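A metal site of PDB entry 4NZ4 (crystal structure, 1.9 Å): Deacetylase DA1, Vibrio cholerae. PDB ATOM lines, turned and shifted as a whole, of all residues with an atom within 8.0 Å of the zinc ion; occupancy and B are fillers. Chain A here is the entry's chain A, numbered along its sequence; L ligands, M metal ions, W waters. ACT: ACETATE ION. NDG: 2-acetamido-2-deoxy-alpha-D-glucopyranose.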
ATOM      1  N   PHE A  13     -20.156  16.908   4.253  1.00  0.00           N
ATOM      2  CA  PHE A  13     -18.933  17.280   3.589  1.00  0.00           C
ATOM      3  C   PHE A  13     -18.082  16.032   3.428  1.00  0.00           C
ATOM      4  O   PHE A  13     -17.813  15.349   4.407  1.00  0.00           O
ATOM      5  CB  PHE A  13     -18.213  18.343   4.437  1.00  0.00           C
ATOM      6  CG  PHE A  13     -18.889  19.658   4.436  1.00  0.00           C
ATOM      7  CD1 PHE A  13     -18.564  20.625   3.485  1.00  0.00           C
ATOM      8  CD2 PHE A  13     -19.819  19.982   5.404  1.00  0.00           C
ATOM      9  CE1 PHE A  13     -19.223  21.854   3.476  1.00  0.00           C
ATOM     10  CE2 PHE A  13     -20.482  21.188   5.389  1.00  0.00           C
ATOM     11  CZ  PHE A  13     -20.156  22.137   4.439  1.00  0.00           C
ATOM     12  N   ASP A  14     -17.725  15.700   2.178  1.00  0.00           N
ATOM     13  CA  ASP A  14     -16.895  14.547   1.860  1.00  0.00           C
ATOM     14  C   ASP A  14     -15.463  14.868   1.503  1.00  0.00           C
ATOM     15  O   ASP A  14     -15.197  15.895   0.917  1.00  0.00           O
ATOM     16  CB  ASP A  14     -17.475  13.742   0.670  1.00  0.00           C
ATOM     17  CG  ASP A  14     -18.723  12.987   1.048  1.00  0.00           C
ATOM     18  OD1 ASP A  14     -19.303  13.319   2.130  1.00  0.00           O
ATOM     19  OD2 ASP A  14     -19.152  12.095   0.261  1.00  0.00           O
ATOM     20  N   ASP A  15     -14.567  13.950   1.856  1.00  0.00           N
ATOM     21  CA  ASP A  15     -13.201  13.853   1.341  1.00  0.00           C
ATOM     22  C   ASP A  15     -12.155  14.654   2.128  1.00  0.00           C
ATOM     23  O   ASP A  15     -10.969  14.601   1.844  1.00  0.00           O
ATOM     24  CB  ASP A  15     -13.092  14.224  -0.164  1.00  0.00           C
ATOM     25  CG  ASP A  15     -13.879  13.299  -1.099  1.00  0.00           C
ATOM     26  OD1 ASP A  15     -14.797  12.556  -0.690  1.00  0.00           O
ATOM     27  OD2 ASP A  15     -13.605  13.361  -2.312  1.00  0.00           O
ATOM     28  N   GLY A  16     -12.600  15.387   3.144  1.00  0.00           N
ATOM     29  CA  GLY A  16     -11.700  15.886   4.160  1.00  0.00           C
ATOM     30  C   GLY A  16     -11.030  14.769   4.921  1.00  0.00           C
ATOM     31  O   GLY A  16     -11.276  13.608   4.644  1.00  0.00           O
ATOM     32  N   TYR A  38     -17.644  13.278   6.252  1.00  0.00           N
ATOM     33  CA  TYR A  38     -17.261  11.937   5.846  1.00  0.00           C
ATOM     34  C   TYR A  38     -15.822  11.945   5.396  1.00  0.00           C
ATOM     35  O   TYR A  38     -15.504  12.381   4.275  1.00  0.00           O
ATOM     36  CB  TYR A  38     -18.176  11.452   4.732  1.00  0.00           C
ATOM     37  CG  TYR A  38     -19.526  11.128   5.284  1.00  0.00           C
ATOM     38  CD1 TYR A  38     -19.745   9.932   5.954  1.00  0.00           C
ATOM     39  CD2 TYR A  38     -20.562  12.035   5.188  1.00  0.00           C
ATOM     40  CE1 TYR A  38     -21.010   9.619   6.465  1.00  0.00           C
ATOM     41  CE2 TYR A  38     -21.792  11.759   5.700  1.00  0.00           C
ATOM     42  CZ  TYR A  38     -22.014  10.545   6.342  1.00  0.00           C
ATOM     43  OH  TYR A  38     -23.259  10.308   6.827  1.00  0.00           O
ATOM     44  N   ASN A  40     -11.785  10.803   4.732  1.00  0.00           N
ATOM     45  CA  ASN A  40     -10.753   9.892   4.265  1.00  0.00           C
ATOM     46  C   ASN A  40      -9.453  10.199   4.985  1.00  0.00           C
ATOM     47  O   ASN A  40      -8.869  11.259   4.781  1.00  0.00           O
ATOM     48  CB  ASN A  40     -10.503  10.087   2.766  1.00  0.00           C
ATOM     49  CG  ASN A  40     -11.734   9.893   1.948  1.00  0.00           C
ATOM     50  OD1 ASN A  40     -12.144  10.791   1.226  1.00  0.00           O
ATOM     51  ND2 ASN A  40     -12.333   8.702   2.021  1.00  0.00           N
ATOM     52  N   HIS A  72     -15.519   7.653   5.350  1.00  0.00           N
ATOM     53  CA  HIS A  72     -15.626   7.668   3.878  1.00  0.00           C
ATOM     54  C   HIS A  72     -14.603   6.701   3.235  1.00  0.00           C
ATOM     55  O   HIS A  72     -14.373   6.731   2.008  1.00  0.00           O
ATOM     56  CB  HIS A  72     -15.422   9.109   3.390  1.00  0.00           C
ATOM     57  CG  HIS A  72     -15.924   9.365   2.005  1.00  0.00           C
ATOM     58  ND1 HIS A  72     -17.050   8.760   1.496  1.00  0.00           N
ATOM     59  CD2 HIS A  72     -15.466  10.190   1.032  1.00  0.00           C
ATOM     60  CE1 HIS A  72     -17.257   9.178   0.257  1.00  0.00           C
ATOM     61  NE2 HIS A  72     -16.307  10.047  -0.044  1.00  0.00           N
ATOM     62  N   SER A  73     -14.008   5.846   4.079  1.00  0.00           N
ATOM     63  CA  SER A  73     -12.914   4.895   3.733  1.00  0.00           C
ATOM     64  C   SER A  73     -11.600   5.603   3.812  1.00  0.00           C
ATOM     65  O   SER A  73     -11.550   6.832   3.708  1.00  0.00           O
ATOM     66  CB  SER A  73     -13.055   4.209   2.342  1.00  0.00           C
ATOM     67  OG  SER A  73     -12.608   5.032   1.284  1.00  0.00           O
ATOM     68  N   HIS A  76     -10.488   6.630  -0.262  1.00  0.00           N
ATOM     69  CA  HIS A  76     -11.475   6.876  -1.313  1.00  0.00           C
ATOM     70  C   HIS A  76     -11.375   5.863  -2.466  1.00  0.00           C
ATOM     71  O   HIS A  76     -11.728   6.192  -3.588  1.00  0.00           O
ATOM     72  CB  HIS A  76     -11.267   8.287  -1.901  1.00  0.00           C
ATOM     73  CG  HIS A  76     -12.536   8.966  -2.251  1.00  0.00           C
ATOM     74  ND1 HIS A  76     -13.140   8.836  -3.483  1.00  0.00           N
ATOM     75  CD2 HIS A  76     -13.323   9.799  -1.524  1.00  0.00           C
ATOM     76  CE1 HIS A  76     -14.268   9.536  -3.482  1.00  0.00           C
ATOM     77  NE2 HIS A  76     -14.385  10.138  -2.309  1.00  0.00           N
ATOM     78  N   ARG A 141     -20.113   6.321   4.292  1.00  0.00           N
ATOM     79  CA  ARG A 141     -20.680   6.650   2.979  1.00  0.00           C
ATOM     80  C   ARG A 141     -19.650   6.187   1.979  1.00  0.00           C
ATOM     81  O   ARG A 141     -18.449   6.490   2.127  1.00  0.00           O
ATOM     82  CB  ARG A 141     -20.940   8.152   2.820  1.00  0.00           C
ATOM     83  CG  ARG A 141     -21.259   8.559   1.405  1.00  0.00           C
ATOM     84  CD  ARG A 141     -21.488  10.006   1.293  1.00  0.00           C
ATOM     85  NE  ARG A 141     -22.768  10.444   1.837  1.00  0.00           N
ATOM     86  CZ  ARG A 141     -23.035  11.705   2.157  1.00  0.00           C
ATOM     87  NH1 ARG A 141     -22.083  12.612   2.054  1.00  0.00           N
ATOM     88  NH2 ARG A 141     -24.209  12.068   2.602  1.00  0.00           N
ATOM     89  N   LEU A 142     -20.121   5.485   0.957  1.00  0.00           N
ATOM     90  CA  LEU A 142     -19.205   4.888  -0.002  1.00  0.00           C
ATOM     91  C   LEU A 142     -18.713   5.906  -1.000  1.00  0.00           C
ATOM     92  O   LEU A 142     -19.505   6.684  -1.528  1.00  0.00           O
ATOM     93  CB  LEU A 142     -19.854   3.756  -0.787  1.00  0.00           C
ATOM     94  CG  LEU A 142     -19.549   2.361  -0.245  1.00  0.00           C
ATOM     95  CD1 LEU A 142     -20.165   2.209   1.134  1.00  0.00           C
ATOM     96  CD2 LEU A 142     -20.085   1.309  -1.191  1.00  0.00           C
ATOM     97  N   PRO A 143     -17.416   5.878  -1.278  1.00  0.00           N
ATOM     98  CA  PRO A 143     -16.876   6.671  -2.391  1.00  0.00           C
ATOM     99  C   PRO A 143     -17.668   6.499  -3.680  1.00  0.00           C
ATOM    100  O   PRO A 143     -17.993   5.360  -4.033  1.00  0.00           O
ATOM    101  CB  PRO A 143     -15.463   6.098  -2.535  1.00  0.00           C
ATOM    102  CG  PRO A 143     -15.054   5.778  -1.114  1.00  0.00           C
ATOM    103  CD  PRO A 143     -16.355   5.233  -0.491  1.00  0.00           C
ATOM    104  N   TYR A 144     -18.018   7.629  -4.309  1.00  0.00           N
ATOM    105  CA  TYR A 144     -18.650   7.681  -5.621  1.00  0.00           C
ATOM    106  C   TYR A 144     -20.100   7.259  -5.659  1.00  0.00           C
ATOM    107  O   TYR A 144     -20.753   7.355  -6.697  1.00  0.00           O
ATOM    108  CB  TYR A 144     -17.905   6.800  -6.634  1.00  0.00           C
ATOM    109  CG  TYR A 144     -16.450   6.996  -6.569  1.00  0.00           C
ATOM    110  CD1 TYR A 144     -15.893   8.226  -6.888  1.00  0.00           C
ATOM    111  CD2 TYR A 144     -15.623   5.971  -6.139  1.00  0.00           C
ATOM    112  CE1 TYR A 144     -14.543   8.404  -6.822  1.00  0.00           C
ATOM    113  CE2 TYR A 144     -14.274   6.161  -6.052  1.00  0.00           C
ATOM    114  CZ  TYR A 144     -13.744   7.388  -6.381  1.00  0.00           C
ATOM    115  OH  TYR A 144     -12.399   7.573  -6.286  1.00  0.00           O
ATOM    116  N   THR A 145     -20.621   6.797  -4.522  1.00  0.00           N
ATOM    117  CA  THR A 145     -21.798   5.954  -4.553  1.00  0.00           C
ATOM    118  C   THR A 145     -22.969   6.474  -3.727  1.00  0.00           C
ATOM    119  O   THR A 145     -22.922   6.561  -2.485  1.00  0.00           O
ATOM    120  CB  THR A 145     -21.422   4.523  -4.105  1.00  0.00           C
ATOM    121  OG1 THR A 145     -20.369   4.024  -4.929  1.00  0.00           O
ATOM    122  CG2 THR A 145     -22.599   3.597  -4.198  1.00  0.00           C
ATOM    123  N   TRP A 204     -27.128  10.801  -0.670  1.00  0.00           N
ATOM    124  CA  TRP A 204     -27.448  12.221  -0.625  1.00  0.00           C
ATOM    125  C   TRP A 204     -28.650  12.503  -1.489  1.00  0.00           C
ATOM    126  O   TRP A 204     -28.975  11.720  -2.365  1.00  0.00           O
ATOM    127  CB  TRP A 204     -26.247  13.046  -1.069  1.00  0.00           C
ATOM    128  CG  TRP A 204     -25.718  12.752  -2.452  1.00  0.00           C
ATOM    129  CD1 TRP A 204     -26.028  13.407  -3.611  1.00  0.00           C
ATOM    130  CD2 TRP A 204     -24.777  11.727  -2.803  1.00  0.00           C
ATOM    131  NE1 TRP A 204     -25.328  12.864  -4.669  1.00  0.00           N
ATOM    132  CE2 TRP A 204     -24.561  11.829  -4.202  1.00  0.00           C
ATOM    133  CE3 TRP A 204     -24.100  10.742  -2.082  1.00  0.00           C
ATOM    134  CZ2 TRP A 204     -23.700  10.990  -4.882  1.00  0.00           C
ATOM    135  CZ3 TRP A 204     -23.244   9.915  -2.755  1.00  0.00           C
ATOM    136  CH2 TRP A 204     -23.068  10.025  -4.147  1.00  0.00           C
ATOM    137  N   LEU A 268     -24.837  16.760  -0.181  1.00  0.00           N
ATOM    138  CA  LEU A 268     -23.477  16.328  -0.315  1.00  0.00           C
ATOM    139  C   LEU A 268     -22.737  17.532  -0.838  1.00  0.00           C
ATOM    140  O   LEU A 268     -23.215  18.244  -1.738  1.00  0.00           O
ATOM    141  CB  LEU A 268     -23.338  15.175  -1.327  1.00  0.00           C
ATOM    142  CG  LEU A 268     -21.937  14.918  -1.900  1.00  0.00           C
ATOM    143  CD1 LEU A 268     -20.962  14.404  -0.847  1.00  0.00           C
ATOM    144  CD2 LEU A 268     -22.023  13.973  -3.078  1.00  0.00           C
ATOM    145  N   THR A 269     -21.570  17.770  -0.269  1.00  0.00           N
ATOM    146  CA  THR A 269     -20.577  18.578  -0.954  1.00  0.00           C
ATOM    147  C   THR A 269     -19.178  18.157  -0.557  1.00  0.00           C
ATOM    148  O   THR A 269     -18.988  17.139   0.128  1.00  0.00           O
ATOM    149  CB  THR A 269     -20.840  20.079  -0.762  1.00  0.00           C
ATOM    150  OG1 THR A 269     -20.045  20.829  -1.703  1.00  0.00           O
ATOM    151  CG2 THR A 269     -20.557  20.509   0.666  1.00  0.00           C
ATOM    152  N   HIS A 270     -18.184  18.904  -1.041  1.00  0.00           N
ATOM    153  CA  HIS A 270     -16.805  18.548  -0.837  1.00  0.00           C
ATOM    154  C   HIS A 270     -16.024  19.714  -0.293  1.00  0.00           C
ATOM    155  O   HIS A 270     -16.071  20.802  -0.850  1.00  0.00           O
ATOM    156  CB  HIS A 270     -16.172  18.065  -2.158  1.00  0.00           C
ATOM    157  CG  HIS A 270     -16.717  16.753  -2.653  1.00  0.00           C
ATOM    158  ND1 HIS A 270     -17.927  16.638  -3.327  1.00  0.00           N
ATOM    159  CD2 HIS A 270     -16.205  15.509  -2.616  1.00  0.00           C
ATOM    160  CE1 HIS A 270     -18.136  15.375  -3.643  1.00  0.00           C
ATOM    161  NE2 HIS A 270     -17.101  14.669  -3.237  1.00  0.00           N
ATOM    162  N   PHE A 272     -12.999  20.376  -0.494  1.00  0.00           N
ATOM    163  CA  PHE A 272     -12.032  20.929  -1.447  1.00  0.00           C
ATOM    164  C   PHE A 272     -12.630  21.973  -2.396  1.00  0.00           C
ATOM    165  O   PHE A 272     -11.881  22.689  -3.065  1.00  0.00           O
ATOM    166  CB  PHE A 272     -11.266  19.844  -2.229  1.00  0.00           C
ATOM    167  CG  PHE A 272     -12.118  18.940  -3.120  1.00  0.00           C
ATOM    168  CD1 PHE A 272     -12.893  19.450  -4.158  1.00  0.00           C
ATOM    169  CD2 PHE A 272     -12.096  17.561  -2.923  1.00  0.00           C
ATOM    170  CE1 PHE A 272     -13.660  18.604  -4.948  1.00  0.00           C
ATOM    171  CE2 PHE A 272     -12.854  16.716  -3.735  1.00  0.00           C
ATOM    172  CZ  PHE A 272     -13.628  17.238  -4.738  1.00  0.00           C
HETATM  173  C   ACT L   1     -18.361  10.858  -2.558  1.00  0.00           C
HETATM  174  O   ACT L   1     -17.539  10.043  -3.012  1.00  0.00           O
HETATM  175  OXT ACT L   1     -17.925  11.870  -1.925  1.00  0.00           O
HETATM  176  CH3 ACT L   1     -19.819  10.589  -2.756  1.00  0.00           C
HETATM  177  C1  NDG L   2     -12.889  13.399  -6.452  1.00  0.00           C
HETATM  178  C2  NDG L   2     -11.837  14.387  -6.994  1.00  0.00           C
HETATM  179  C3  NDG L   2     -10.436  13.798  -6.972  1.00  0.00           C
HETATM  180  C4  NDG L   2     -10.121  13.257  -5.581  1.00  0.00           C
HETATM  181  C5  NDG L   2     -11.192  12.249  -5.180  1.00  0.00           C
HETATM  182  C6  NDG L   2     -10.944  11.762  -3.745  1.00  0.00           C
HETATM  183  C7  NDG L   2     -12.151  16.196  -8.696  1.00  0.00           C
HETATM  184  C8  NDG L   2     -12.647  16.411 -10.110  1.00  0.00           C
HETATM  185  O5  NDG L   2     -12.484  12.880  -5.197  1.00  0.00           O
HETATM  186  O3  NDG L   2      -9.599  14.902  -7.264  1.00  0.00           O
HETATM  187  O4  NDG L   2      -8.861  12.600  -5.595  1.00  0.00           O
HETATM  188  O6  NDG L   2     -11.194  12.803  -2.779  1.00  0.00           O
HETATM  189  O7  NDG L   2     -11.737  17.115  -7.972  1.00  0.00           O
HETATM  190  N2  NDG L   2     -12.198  14.879  -8.319  1.00  0.00           N
HETATM  191  O1  NDG L   2     -13.092  12.369  -7.397  1.00  0.00           O
HETATM  192 ZN    ZN M   1     -15.889  11.203  -1.835  1.00  0.00          ZN
HETATM  193  O   HOH W   1     -15.467  12.472  -3.772  1.00  0.00           O
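The backbone carbonyl oxygen (O) of His 72 sits at hydrogen-bond distance from the side-chain amide nitrogen (ND2) of Asn 40, 2.8 Å away.
N of His 76 sits at hydrogen-bond distance from OG of Ser 73.
The backbone carbonyl oxygen of Arg 141 lies within hydrogen-bond range of a ring nitrogen (ND1) of His 72, at 2.7 Å.
The backbone NH (N) of Asp 14 is in hydrogen-bond range of the backbone carbonyl oxygen (O) of Thr 269.
The side-chain carboxylate (OD1) of Asp 14 lies within salt-bridge range of the guanidinium group (NH1) of Arg 141 (2.9 Å).
N of Asp 15 lies within hydrogen-bond range of O of Tyr 38 (3.0 Å).
The backbone carbonyl oxygen of His 76 sits at hydrogen-bond distance from the side-chain hydroxyl of Tyr 144.
Water W1 lies within hydrogen-bond range of OD2 of Asp 15, NE2 of His 270 and O5 of NDG L2.
The zinc ion is bound by NE2 of His 76, OD1 of Asp 15, OXT of ACT L1, NE2 of His 72, O of ACT L1 and water W1.
The zinc ion has six donor atoms within binding distance.
The side-chain carboxylate of Asp 15 is in hydrogen-bond range of an oxygen (O6) of NDG L2, 2.5 Å away.
Asp 14 touches the zinc ion (CB to ZN, 3.9 Å).
His 270 touches the zinc ion.
Within 4 Å of the zinc ion: Asp 14, Asp 15, His 72, His 76 and His 270.
Along chain A the residues within 4 Å of the zinc ion span positions 14 to 270.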
